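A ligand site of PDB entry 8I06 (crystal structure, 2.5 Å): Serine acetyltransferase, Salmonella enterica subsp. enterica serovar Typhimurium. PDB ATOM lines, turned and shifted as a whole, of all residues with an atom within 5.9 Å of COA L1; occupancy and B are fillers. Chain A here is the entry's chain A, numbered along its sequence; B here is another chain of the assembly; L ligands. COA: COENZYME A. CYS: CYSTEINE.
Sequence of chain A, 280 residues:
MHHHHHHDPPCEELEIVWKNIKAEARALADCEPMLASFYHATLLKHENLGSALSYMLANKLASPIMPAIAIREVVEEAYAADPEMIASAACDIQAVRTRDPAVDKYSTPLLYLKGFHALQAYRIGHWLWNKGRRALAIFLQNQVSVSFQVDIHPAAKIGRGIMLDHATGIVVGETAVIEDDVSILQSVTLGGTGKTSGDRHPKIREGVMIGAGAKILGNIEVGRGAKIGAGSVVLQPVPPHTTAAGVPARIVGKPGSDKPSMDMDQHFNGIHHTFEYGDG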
ATOM      1  N   ASP A 165       8.673   5.523 -20.226  1.00  0.00           N
ATOM      2  CA  ASP A 165       7.430   5.175 -19.500  1.00  0.00           C
ATOM      3  C   ASP A 165       6.711   6.486 -19.574  1.00  0.00           C
ATOM      4  O   ASP A 165       7.375   7.495 -19.644  1.00  0.00           O
ATOM      5  CB  ASP A 165       7.700   4.666 -18.071  1.00  0.00           C
ATOM      6  CG  ASP A 165       7.775   5.777 -17.040  1.00  0.00           C
ATOM      7  OD1 ASP A 165       7.035   5.726 -16.050  1.00  0.00           O
ATOM      8  OD2 ASP A 165       8.578   6.700 -17.236  1.00  0.00           O
ATOM      9  N   HIS A 166       5.410   6.563 -19.679  1.00  0.00           N
ATOM     10  CA  HIS A 166       4.424   5.558 -19.943  1.00  0.00           C
ATOM     11  C   HIS A 166       4.105   6.093 -21.321  1.00  0.00           C
ATOM     12  O   HIS A 166       3.610   7.186 -21.442  1.00  0.00           O
ATOM     13  CB  HIS A 166       3.208   5.873 -19.092  1.00  0.00           C
ATOM     14  CG  HIS A 166       3.505   6.075 -17.656  1.00  0.00           C
ATOM     15  ND1 HIS A 166       3.186   5.151 -16.693  1.00  0.00           N
ATOM     16  CD2 HIS A 166       4.127   7.096 -17.032  1.00  0.00           C
ATOM     17  CE1 HIS A 166       3.611   5.587 -15.521  1.00  0.00           C
ATOM     18  NE2 HIS A 166       4.182   6.774 -15.701  1.00  0.00           N
ATOM     19  N   LEU A 185       8.967  10.960 -20.680  1.00  0.00           N
ATOM     20  CA  LEU A 185       7.632  10.589 -20.242  1.00  0.00           C
ATOM     21  C   LEU A 185       6.571  10.750 -21.378  1.00  0.00           C
ATOM     22  O   LEU A 185       6.871  10.865 -22.573  1.00  0.00           O
ATOM     23  CB  LEU A 185       7.353  11.294 -18.936  1.00  0.00           C
ATOM     24  CG  LEU A 185       8.239  10.849 -17.747  1.00  0.00           C
ATOM     25  CD1 LEU A 185       9.729  10.687 -17.945  1.00  0.00           C
ATOM     26  CD2 LEU A 185       8.077  11.893 -16.672  1.00  0.00           C
ATOM     27  N   GLN A 186       5.320  10.667 -21.011  1.00  0.00           N
ATOM     28  CA  GLN A 186       4.257  10.690 -21.975  1.00  0.00           C
ATOM     29  C   GLN A 186       4.120  12.050 -22.638  1.00  0.00           C
ATOM     30  O   GLN A 186       4.353  13.064 -22.025  1.00  0.00           O
ATOM     31  CB  GLN A 186       2.935  10.306 -21.302  1.00  0.00           C
ATOM     32  CG  GLN A 186       2.509  11.163 -20.095  1.00  0.00           C
ATOM     33  CD  GLN A 186       3.178  10.705 -18.817  1.00  0.00           C
ATOM     34  OE1 GLN A 186       4.258  10.094 -18.843  1.00  0.00           O
ATOM     35  NE2 GLN A 186       2.548  11.003 -17.686  1.00  0.00           N
ATOM     36  N   MET A 209      16.426  14.363 -18.474  1.00  0.00           N
ATOM     37  CA  MET A 209      15.092  13.955 -18.038  1.00  0.00           C
ATOM     38  C   MET A 209      14.069  14.891 -18.704  1.00  0.00           C
ATOM     39  O   MET A 209      14.110  16.106 -18.542  1.00  0.00           O
ATOM     40  CB  MET A 209      15.037  14.041 -16.514  1.00  0.00           C
ATOM     41  CG  MET A 209      13.854  13.310 -15.876  1.00  0.00           C
ATOM     42  SD  MET A 209      12.239  14.114 -16.134  1.00  0.00           S
ATOM     43  CE  MET A 209      12.396  15.700 -15.302  1.00  0.00           C
ATOM     44  N   ILE A 210      13.142  14.340 -19.477  1.00  0.00           N
ATOM     45  CA  ILE A 210      12.162  15.171 -20.163  1.00  0.00           C
ATOM     46  C   ILE A 210      10.801  14.869 -19.584  1.00  0.00           C
ATOM     47  O   ILE A 210      10.330  13.743 -19.662  1.00  0.00           O
ATOM     48  CB  ILE A 210      12.138  14.924 -21.659  1.00  0.00           C
ATOM     49  CG1 ILE A 210      13.574  14.956 -22.228  1.00  0.00           C
ATOM     50  CG2 ILE A 210      11.252  15.977 -22.328  1.00  0.00           C
ATOM     51  CD1 ILE A 210      13.648  14.872 -23.737  1.00  0.00           C
ATOM     52  N   GLY A 211      10.185  15.877 -19.019  1.00  0.00           N
ATOM     53  CA  GLY A 211       8.936  15.712 -18.324  1.00  0.00           C
ATOM     54  C   GLY A 211       7.759  15.673 -19.261  1.00  0.00           C
ATOM     55  O   GLY A 211       7.872  16.062 -20.411  1.00  0.00           O
ATOM     56  N   ALA A 212       6.635  15.224 -18.728  1.00  0.00           N
ATOM     57  CA  ALA A 212       5.410  14.925 -19.472  1.00  0.00           C
ATOM     58  C   ALA A 212       4.946  16.136 -20.217  1.00  0.00           C
ATOM     59  O   ALA A 212       4.922  17.242 -19.658  1.00  0.00           O
ATOM     60  CB  ALA A 212       4.327  14.487 -18.526  1.00  0.00           C
ATOM     61  N   LYS A 227      17.247  18.999 -17.111  1.00  0.00           N
ATOM     62  CA  LYS A 227      15.902  18.594 -16.833  1.00  0.00           C
ATOM     63  C   LYS A 227      14.929  19.505 -17.519  1.00  0.00           C
ATOM     64  O   LYS A 227      15.017  20.705 -17.367  1.00  0.00           O
ATOM     65  CB  LYS A 227      15.681  18.692 -15.359  1.00  0.00           C
ATOM     66  CG  LYS A 227      16.434  17.652 -14.578  1.00  0.00           C
ATOM     67  CD  LYS A 227      16.416  17.979 -13.100  1.00  0.00           C
ATOM     68  CE  LYS A 227      17.045  16.858 -12.317  1.00  0.00           C
ATOM     69  NZ  LYS A 227      17.158  17.260 -10.895  1.00  0.00           N
ATOM     70  N   ILE A 228      13.965  18.927 -18.242  1.00  0.00           N
ATOM     71  CA  ILE A 228      12.909  19.675 -18.940  1.00  0.00           C
ATOM     72  C   ILE A 228      11.595  19.474 -18.185  1.00  0.00           C
ATOM     73  O   ILE A 228      11.116  18.369 -18.019  1.00  0.00           O
ATOM     74  CB  ILE A 228      12.714  19.222 -20.390  1.00  0.00           C
ATOM     75  CG1 ILE A 228      14.053  19.191 -21.151  1.00  0.00           C
ATOM     76  CG2 ILE A 228      11.694  20.098 -21.117  1.00  0.00           C
ATOM     77  CD1 ILE A 228      14.818  20.503 -21.118  1.00  0.00           C
ATOM     78  N   GLY A 229      11.043  20.566 -17.690  1.00  0.00           N
ATOM     79  CA  GLY A 229       9.808  20.539 -16.914  1.00  0.00           C
ATOM     80  C   GLY A 229       8.643  20.033 -17.723  1.00  0.00           C
ATOM     81  O   GLY A 229       8.544  20.285 -18.918  1.00  0.00           O
ATOM     82  N   ALA A 230       7.751  19.297 -17.074  1.00  0.00           N
ATOM     83  CA  ALA A 230       6.521  18.894 -17.685  1.00  0.00           C
ATOM     84  C   ALA A 230       5.842  20.119 -18.264  1.00  0.00           C
ATOM     85  O   ALA A 230       5.859  21.144 -17.665  1.00  0.00           O
ATOM     86  CB  ALA A 230       5.608  18.247 -16.655  1.00  0.00           C
ATOM     87  N   GLY A 231       5.216  19.995 -19.418  1.00  0.00           N
ATOM     88  CA  GLY A 231       4.455  21.094 -20.007  1.00  0.00           C
ATOM     89  C   GLY A 231       5.297  22.080 -20.786  1.00  0.00           C
ATOM     90  O   GLY A 231       4.775  22.996 -21.360  1.00  0.00           O
ATOM     91  N   SER A 232       6.600  21.902 -20.840  1.00  0.00           N
ATOM     92  CA  SER A 232       7.434  22.934 -21.392  1.00  0.00           C
ATOM     93  C   SER A 232       7.359  22.963 -22.894  1.00  0.00           C
ATOM     94  O   SER A 232       7.189  21.934 -23.511  1.00  0.00           O
ATOM     95  CB  SER A 232       8.892  22.678 -21.014  1.00  0.00           C
ATOM     96  OG  SER A 232       9.064  22.811 -19.643  1.00  0.00           O
ATOM     97  N   THR A 243      17.879  23.231 -15.490  1.00  0.00           N
ATOM     98  CA  THR A 243      16.464  22.957 -15.575  1.00  0.00           C
ATOM     99  C   THR A 243      15.808  24.045 -16.439  1.00  0.00           C
ATOM    100  O   THR A 243      16.025  25.243 -16.218  1.00  0.00           O
ATOM    101  CB  THR A 243      15.838  22.959 -14.173  1.00  0.00           C
ATOM    102  OG1 THR A 243      16.483  21.975 -13.363  1.00  0.00           O
ATOM    103  CG2 THR A 243      14.378  22.601 -14.235  1.00  0.00           C
ATOM    104  N   ALA A 244      15.052  23.622 -17.442  1.00  0.00           N
ATOM    105  CA  ALA A 244      14.282  24.561 -18.247  1.00  0.00           C
ATOM    106  C   ALA A 244      12.817  24.215 -18.044  1.00  0.00           C
ATOM    107  O   ALA A 244      12.453  23.057 -18.060  1.00  0.00           O
ATOM    108  CB  ALA A 244      14.655  24.454 -19.700  1.00  0.00           C
ATOM    109  N   ALA A 245      11.995  25.225 -17.825  1.00  0.00           N
ATOM    110  CA  ALA A 245      10.562  25.040 -17.637  1.00  0.00           C
ATOM    111  C   ALA A 245       9.826  26.285 -18.107  1.00  0.00           C
ATOM    112  O   ALA A 245      10.370  27.391 -18.078  1.00  0.00           O
ATOM    113  CB  ALA A 245      10.262  24.764 -16.190  1.00  0.00           C
ATOM    114  N   GLY A 246       8.597  26.086 -18.532  1.00  0.00           N
ATOM    115  CA  GLY A 246       7.716  27.171 -18.943  1.00  0.00           C
ATOM    116  C   GLY A 246       7.305  27.095 -20.386  1.00  0.00           C
ATOM    117  O   GLY A 246       7.827  26.278 -21.160  1.00  0.00           O
ATOM    118  N   ARG A 250      12.120  28.856 -19.942  1.00  0.00           N
ATOM    119  CA  ARG A 250      13.297  29.607 -19.482  1.00  0.00           C
ATOM    120  C   ARG A 250      14.142  28.739 -18.545  1.00  0.00           C
ATOM    121  O   ARG A 250      13.626  27.811 -17.919  1.00  0.00           O
ATOM    122  CB  ARG A 250      12.888  30.949 -18.822  1.00  0.00           C
ATOM    123  CG  ARG A 250      12.344  30.913 -17.392  1.00  0.00           C
ATOM    124  CD  ARG A 250      10.802  30.833 -17.325  1.00  0.00           C
ATOM    125  NE  ARG A 250      10.316  30.110 -16.135  1.00  0.00           N
ATOM    126  CZ  ARG A 250       9.033  29.789 -15.874  1.00  0.00           C
ATOM    127  NH1 ARG A 250       8.056  30.168 -16.712  1.00  0.00           N
ATOM    128  NH2 ARG A 250       8.724  29.113 -14.748  1.00  0.00           N
ATOM    129  N   VAL A 252      15.618  27.910 -15.217  1.00  0.00           N
ATOM    130  CA  VAL A 252      15.014  28.243 -13.920  1.00  0.00           C
ATOM    131  C   VAL A 252      15.963  28.084 -12.762  1.00  0.00           C
ATOM    132  O   VAL A 252      15.753  27.254 -11.897  1.00  0.00           O
ATOM    133  CB  VAL A 252      13.658  27.540 -13.633  1.00  0.00           C
ATOM    134  CG1 VAL A 252      12.539  28.213 -14.412  1.00  0.00           C
ATOM    135  CG2 VAL A 252      13.702  26.049 -13.915  1.00  0.00           C
ATOM    136  N   VAL B 171      -2.653   9.409 -17.264  1.00  0.00           N
ATOM    137  CA  VAL B 171      -1.722   8.630 -16.458  1.00  0.00           C
ATOM    138  C   VAL B 171      -1.989   8.907 -14.991  1.00  0.00           C
ATOM    139  O   VAL B 171      -2.039  10.067 -14.543  1.00  0.00           O
ATOM    140  CB  VAL B 171      -0.276   8.948 -16.831  1.00  0.00           C
ATOM    141  CG1 VAL B 171       0.706   8.146 -15.981  1.00  0.00           C
ATOM    142  CG2 VAL B 171      -0.078   8.682 -18.312  1.00  0.00           C
ATOM    143  N   THR B 189      -2.238  13.996 -16.272  1.00  0.00           N
ATOM    144  CA  THR B 189      -1.236  13.258 -15.560  1.00  0.00           C
ATOM    145  C   THR B 189      -1.361  13.543 -14.062  1.00  0.00           C
ATOM    146  O   THR B 189      -1.333  14.700 -13.626  1.00  0.00           O
ATOM    147  CB  THR B 189       0.148  13.653 -16.083  1.00  0.00           C
ATOM    148  OG1 THR B 189       0.282  13.151 -17.426  1.00  0.00           O
ATOM    149  CG2 THR B 189       1.238  13.085 -15.224  1.00  0.00           C
ATOM    150  N   LEU B 190      -1.501  12.476 -13.290  1.00  0.00           N
ATOM    151  CA  LEU B 190      -1.478  12.559 -11.831  1.00  0.00           C
ATOM    152  C   LEU B 190      -0.223  11.847 -11.392  1.00  0.00           C
ATOM    153  O   LEU B 190      -0.237  10.657 -11.088  1.00  0.00           O
ATOM    154  CB  LEU B 190      -2.750  11.961 -11.198  1.00  0.00           C
ATOM    155  CG  LEU B 190      -4.081  12.589 -11.562  1.00  0.00           C
ATOM    156  CD1 LEU B 190      -5.157  12.056 -10.638  1.00  0.00           C
ATOM    157  CD2 LEU B 190      -4.041  14.105 -11.459  1.00  0.00           C
ATOM    158  N   GLY B 191       0.868  12.590 -11.354  1.00  0.00           N
ATOM    159  CA  GLY B 191       2.178  11.993 -11.184  1.00  0.00           C
ATOM    160  C   GLY B 191       3.131  12.653 -10.209  1.00  0.00           C
ATOM    161  O   GLY B 191       2.753  13.518  -9.424  1.00  0.00           O
ATOM    162  N   GLY B 192       4.371  12.202 -10.265  1.00  0.00           N
ATOM    163  CA  GLY B 192       5.411  12.664  -9.366  1.00  0.00           C
ATOM    164  C   GLY B 192       6.237  13.777  -9.946  1.00  0.00           C
ATOM    165  O   GLY B 192       6.247  14.049 -11.135  1.00  0.00           O
ATOM    166  N   THR B 193       6.939  14.422  -9.043  1.00  0.00           N
ATOM    167  CA  THR B 193       7.924  15.433  -9.368  1.00  0.00           C
ATOM    168  C   THR B 193       9.178  14.860 -10.042  1.00  0.00           C
ATOM    169  O   THR B 193       9.819  15.567 -10.845  1.00  0.00           O
ATOM    170  CB  THR B 193       8.256  16.252  -8.119  1.00  0.00           C
ATOM    171  OG1 THR B 193       7.093  17.028  -7.777  1.00  0.00           O
ATOM    172  CG2 THR B 193       9.276  17.239  -8.406  1.00  0.00           C
ATOM    173  N   GLY B 194       9.508  13.606  -9.737  1.00  0.00           N
ATOM    174  CA  GLY B 194      10.790  13.033 -10.099  1.00  0.00           C
ATOM    175  C   GLY B 194      11.753  12.986  -8.929  1.00  0.00           C
ATOM    176  O   GLY B 194      12.769  12.289  -9.001  1.00  0.00           O
ATOM    177  N   LYS B 195      11.424  13.676  -7.840  1.00  0.00           N
ATOM    178  CA  LYS B 195      12.349  13.864  -6.714  1.00  0.00           C
ATOM    179  C   LYS B 195      12.198  12.893  -5.555  1.00  0.00           C
ATOM    180  O   LYS B 195      13.180  12.656  -4.848  1.00  0.00           O
ATOM    181  CB  LYS B 195      12.180  15.262  -6.137  1.00  0.00           C
ATOM    182  CG  LYS B 195      12.458  16.382  -7.102  1.00  0.00           C
ATOM    183  CD  LYS B 195      11.986  17.676  -6.454  1.00  0.00           C
ATOM    184  CE  LYS B 195      12.121  18.876  -7.364  1.00  0.00           C
ATOM    185  NZ  LYS B 195      12.070  20.115  -6.538  1.00  0.00           N
ATOM    186  N   LEU B 217       1.489  17.399 -10.165  1.00  0.00           N
ATOM    187  CA  LEU B 217       2.718  16.718  -9.790  1.00  0.00           C
ATOM    188  C   LEU B 217       3.061  16.893  -8.330  1.00  0.00           C
ATOM    189  O   LEU B 217       3.032  18.008  -7.824  1.00  0.00           O
ATOM    190  CB  LEU B 217       3.871  17.223 -10.623  1.00  0.00           C
ATOM    191  CG  LEU B 217       3.642  17.210 -12.123  1.00  0.00           C
ATOM    192  CD1 LEU B 217       4.902  17.748 -12.792  1.00  0.00           C
ATOM    193  CD2 LEU B 217       3.320  15.803 -12.618  1.00  0.00           C
ATOM    194  N   VAL B 233       0.260  23.075 -15.217  1.00  0.00           N
ATOM    195  CA  VAL B 233       1.199  22.265 -14.470  1.00  0.00           C
ATOM    196  C   VAL B 233       1.069  22.696 -13.005  1.00  0.00           C
ATOM    197  O   VAL B 233       1.549  23.731 -12.630  1.00  0.00           O
ATOM    198  CB  VAL B 233       2.645  22.443 -14.981  1.00  0.00           C
ATOM    199  CG1 VAL B 233       3.588  21.548 -14.194  1.00  0.00           C
ATOM    200  CG2 VAL B 233       2.734  22.107 -16.467  1.00  0.00           C
ATOM    201  N   LEU B 235       1.941  22.493  -9.217  1.00  0.00           N
ATOM    202  CA  LEU B 235       3.032  22.088  -8.322  1.00  0.00           C
ATOM    203  C   LEU B 235       2.754  22.343  -6.857  1.00  0.00           C
ATOM    204  O   LEU B 235       3.398  21.724  -6.004  1.00  0.00           O
ATOM    205  CB  LEU B 235       4.298  22.810  -8.683  1.00  0.00           C
ATOM    206  CG  LEU B 235       4.777  22.582 -10.107  1.00  0.00           C
ATOM    207  CD1 LEU B 235       5.927  23.518 -10.398  1.00  0.00           C
ATOM    208  CD2 LEU B 235       5.159  21.112 -10.291  1.00  0.00           C
ATOM    209  N   VAL B 247       1.295  27.701 -16.223  1.00  0.00           N
ATOM    210  CA  VAL B 247       2.468  26.872 -16.203  1.00  0.00           C
ATOM    211  C   VAL B 247       3.622  27.619 -15.543  1.00  0.00           C
ATOM    212  O   VAL B 247       4.294  28.375 -16.229  1.00  0.00           O
ATOM    213  CB  VAL B 247       2.837  26.473 -17.650  1.00  0.00           C
ATOM    214  CG1 VAL B 247       4.104  25.602 -17.670  1.00  0.00           C
ATOM    215  CG2 VAL B 247       1.651  25.763 -18.320  1.00  0.00           C
ATOM    216  N   PRO B 248       3.888  27.420 -14.250  1.00  0.00           N
ATOM    217  CA  PRO B 248       3.129  26.562 -13.344  1.00  0.00           C
ATOM    218  C   PRO B 248       1.871  27.242 -12.876  1.00  0.00           C
ATOM    219  O   PRO B 248       1.696  28.452 -13.065  1.00  0.00           O
ATOM    220  CB  PRO B 248       4.086  26.373 -12.160  1.00  0.00           C
ATOM    221  CG  PRO B 248       4.957  27.602 -12.150  1.00  0.00           C
ATOM    222  CD  PRO B 248       4.819  28.288 -13.499  1.00  0.00           C
HETATM  223  N1A COA L   1       6.841  24.064 -15.306  1.00  0.00           N
HETATM  224  C2A COA L   1       7.023  25.351 -14.956  1.00  0.00           C
HETATM  225  N3A COA L   1       7.706  25.731 -13.868  1.00  0.00           N
HETATM  226  C4A COA L   1       8.244  24.804 -13.050  1.00  0.00           C
HETATM  227  C5A COA L   1       8.101  23.384 -13.359  1.00  0.00           C
HETATM  228  C6A COA L   1       7.349  23.051 -14.577  1.00  0.00           C
HETATM  229  N6A COA L   1       7.190  21.757 -14.942  1.00  0.00           N
HETATM  230  N7A COA L   1       8.767  22.669 -12.415  1.00  0.00           N
HETATM  231  C8A COA L   1       9.267  23.587 -11.560  1.00  0.00           C
HETATM  232  N9A COA L   1       8.962  24.846 -11.947  1.00  0.00           N
HETATM  233  C1B COA L   1       9.365  26.090 -11.257  1.00  0.00           C
HETATM  234  C2B COA L   1       9.106  26.135  -9.748  1.00  0.00           C
HETATM  235  O2B COA L   1       7.817  26.703  -9.437  1.00  0.00           O
HETATM  236  C3B COA L   1      10.276  26.968  -9.284  1.00  0.00           C
HETATM  237  O3B COA L   1       9.979  28.375  -9.388  1.00  0.00           O
HETATM  238  P3B COA L   1      10.458  29.493  -8.285  1.00  0.00           P
HETATM  239  O7A COA L   1       9.853  30.722  -8.929  1.00  0.00           O
HETATM  240  O8A COA L   1      11.963  29.482  -8.266  1.00  0.00           O
HETATM  241  O9A COA L   1       9.868  28.980  -7.007  1.00  0.00           O
HETATM  242  C4B COA L   1      11.403  26.648 -10.247  1.00  0.00           C
HETATM  243  O4B COA L   1      10.778  26.197 -11.442  1.00  0.00           O
HETATM  244  C5B COA L   1      12.387  25.579  -9.763  1.00  0.00           C
HETATM  245  O5B COA L   1      11.701  24.420  -9.299  1.00  0.00           O
HETATM  246  P1A COA L   1      12.524  23.154  -8.764  1.00  0.00           P
HETATM  247  O1A COA L   1      11.495  22.199  -8.301  1.00  0.00           O
HETATM  248  O2A COA L   1      13.562  23.677  -7.857  1.00  0.00           O
HETATM  249  O3A COA L   1      13.197  22.647 -10.136  1.00  0.00           O
HETATM  250  P2A COA L   1      14.085  21.335 -10.389  1.00  0.00           P
HETATM  251  O4A COA L   1      15.384  21.638 -11.068  1.00  0.00           O
HETATM  252  O5A COA L   1      14.011  20.397  -9.239  1.00  0.00           O
HETATM  253  O6A COA L   1      13.280  20.522 -11.522  1.00  0.00           O
HETATM  254  CBP COA L   1      11.217  19.582 -12.488  1.00  0.00           C
HETATM  255  CCP COA L   1      11.985  19.953 -11.231  1.00  0.00           C
HETATM  256  CDP COA L   1      11.238  20.757 -13.454  1.00  0.00           C
HETATM  257  CEP COA L   1      11.898  18.384 -13.135  1.00  0.00           C
HETATM  258  CAP COA L   1       9.800  19.160 -12.078  1.00  0.00           C
HETATM  259  OAP COA L   1       9.100  20.267 -11.501  1.00  0.00           O
HETATM  260  C9P COA L   1       9.045  18.535 -13.258  1.00  0.00           C
HETATM  261  O9P COA L   1       8.580  19.241 -14.131  1.00  0.00           O
HETATM  262  N8P COA L   1       8.946  17.191 -13.266  1.00  0.00           N
HETATM  263  C7P COA L   1       8.260  16.444 -14.299  1.00  0.00           C
HETATM  264  C6P COA L   1       7.791  15.035 -13.862  1.00  0.00           C
HETATM  265  C5P COA L   1       6.865  14.470 -14.910  1.00  0.00           C
HETATM  266  O5P COA L   1       6.854  14.978 -16.020  1.00  0.00           O
HETATM  267  N4P COA L   1       6.063  13.420 -14.801  1.00  0.00           N
HETATM  268  C3P COA L   1       5.974  12.344 -13.849  1.00  0.00           C
HETATM  269  C2P COA L   1       4.516  11.874 -13.886  1.00  0.00           C
HETATM  270  S1P COA L   1       4.119  10.505 -15.019  1.00  0.00           S
HETATM  271  N   CYS L   2       5.579   6.370 -12.994  1.00  0.00           N
HETATM  272  CA  CYS L   2       6.514   7.028 -12.088  1.00  0.00           C
HETATM  273  C   CYS L   2       5.997   7.000 -10.647  1.00  0.00           C
HETATM  274  O   CYS L   2       6.351   7.881  -9.846  1.00  0.00           O
HETATM  275  CB  CYS L   2       6.752   8.474 -12.530  1.00  0.00           C
HETATM  276  SG  CYS L   2       5.591   9.634 -11.797  1.00  0.00           S
HETATM  277  OXT CYS L   2       5.221   6.111 -10.252  1.00  0.00           O
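OG1 of Thr 243 lies within hydrogen-bond range of O4A of COA L1, at 2.6 Å.
The backbone NH of Ala 212 sits at hydrogen-bond distance from an oxygen (O5P) of COA L1, 2.7 Å away.
An oxygen (O1A) of COA L1 lies within salt-bridge range of the side-chain amino group (NZ) of Lys 195 of chain B (2.8 Å).
The backbone carbonyl oxygen (O) of Thr 193 of chain B sits at hydrogen-bond distance from a nitrogen (N8P) of COA L1 (3.0 Å).
N of Ala 230 sits at hydrogen-bond distance from O9P of COA L1, at 3.1 Å.
O of Ala 230 is in hydrogen-bond range of N6A of COA L1 (3.1 Å).
A sulfur (S1P) of COA L1 sits close to the side-chain amide nitrogen (NE2) of Gln 186 (3.1 Å).
A sulfur (S1P) of COA L1 sits close to a ring nitrogen (NE2) of His 166 (3.8 Å).
The backbone NH (N) of Gly 192 of chain B sits close to a sulfur (SG) of CYS L2 (3.2 Å).
NE2 of His 166 sits at hydrogen-bond distance from N of CYS L2 (3.1 Å).
The side-chain carboxylate of Asp 165 lies within salt-bridge range of a nitrogen (N) of CYS L2 (3.4 Å).
Leu 185 touches COA L1 (CD2 to N4P, 3.1 Å).
Met 209 touches COA L1 (CE to CEP, 3.5 Å).
CA of Gly 211 touches O5P of COA L1, 3.2 Å away.
Gly 229 touches COA L1.
CB of Ala 245 touches C2A of COA L1, at 3.5 Å.
Gly 246 touches COA L1.
NH2 of Arg 250 touches N3A of COA L1 (3.6 Å).
Val 252 touches COA L1.
Thr 189 of chain B touches COA L1 (CG2 to C2P, 3.7 Å).
CA of Gly 191 of chain B touches C2P of COA L1 (3.6 Å).
O of Gly 192 of chain B touches C3P of COA L1 (3.2 Å).
CD1 of Leu 217 of chain B touches C7P of COA L1 (3.9 Å).
Val 233 of chain B touches COA L1.
Leu 235 of chain B touches COA L1.
CG1 of Val 247 of chain B touches N1A of COA L1, at 3.9 Å.
Pro 248 of chain B touches COA L1 (CG to N3A, 3.7 Å).
Hydrophobic or aromatic side chains that line COA L1: His 166, Leu 185, Met 209, Ala 212, Ala 230, Ala 245, Val 252, Leu 217 of chain B, Val 233 of chain B, Leu 235 of chain B, Val 247 of chain B and Pro 248 of chain B.
O of Thr 243 sits at hydrogen-bond distance from N of Val 252, 2.9 Å away.
OG1 of Thr 189 of chain B lies within hydrogen-bond range of NE2 of Gln 186.
N of Leu 185 lies within hydrogen-bond range of O of Ile 210 (3.3 Å).
N of Gly 211 is in hydrogen-bond range of O of Ile 228, 2.8 Å away.
O of Gly 229 sits at hydrogen-bond distance from OG of Ser 232 (2.7 Å).
The backbone NH of Arg 250 sits at hydrogen-bond distance from the backbone carbonyl oxygen of Ala 245 (2.9 Å).
A ring nitrogen (NE2) of His 166 sits at hydrogen-bond distance from the side-chain carboxylate of Asp 165.
The side-chain hydroxyl (OG) of Ser 232 sits at hydrogen-bond distance from the backbone NH (N) of Gly 246 (3.5 Å).
A sulfur (SG) of CYS L2 sits close to a sulfur (S1P) of COA L1, 3.6 Å away.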
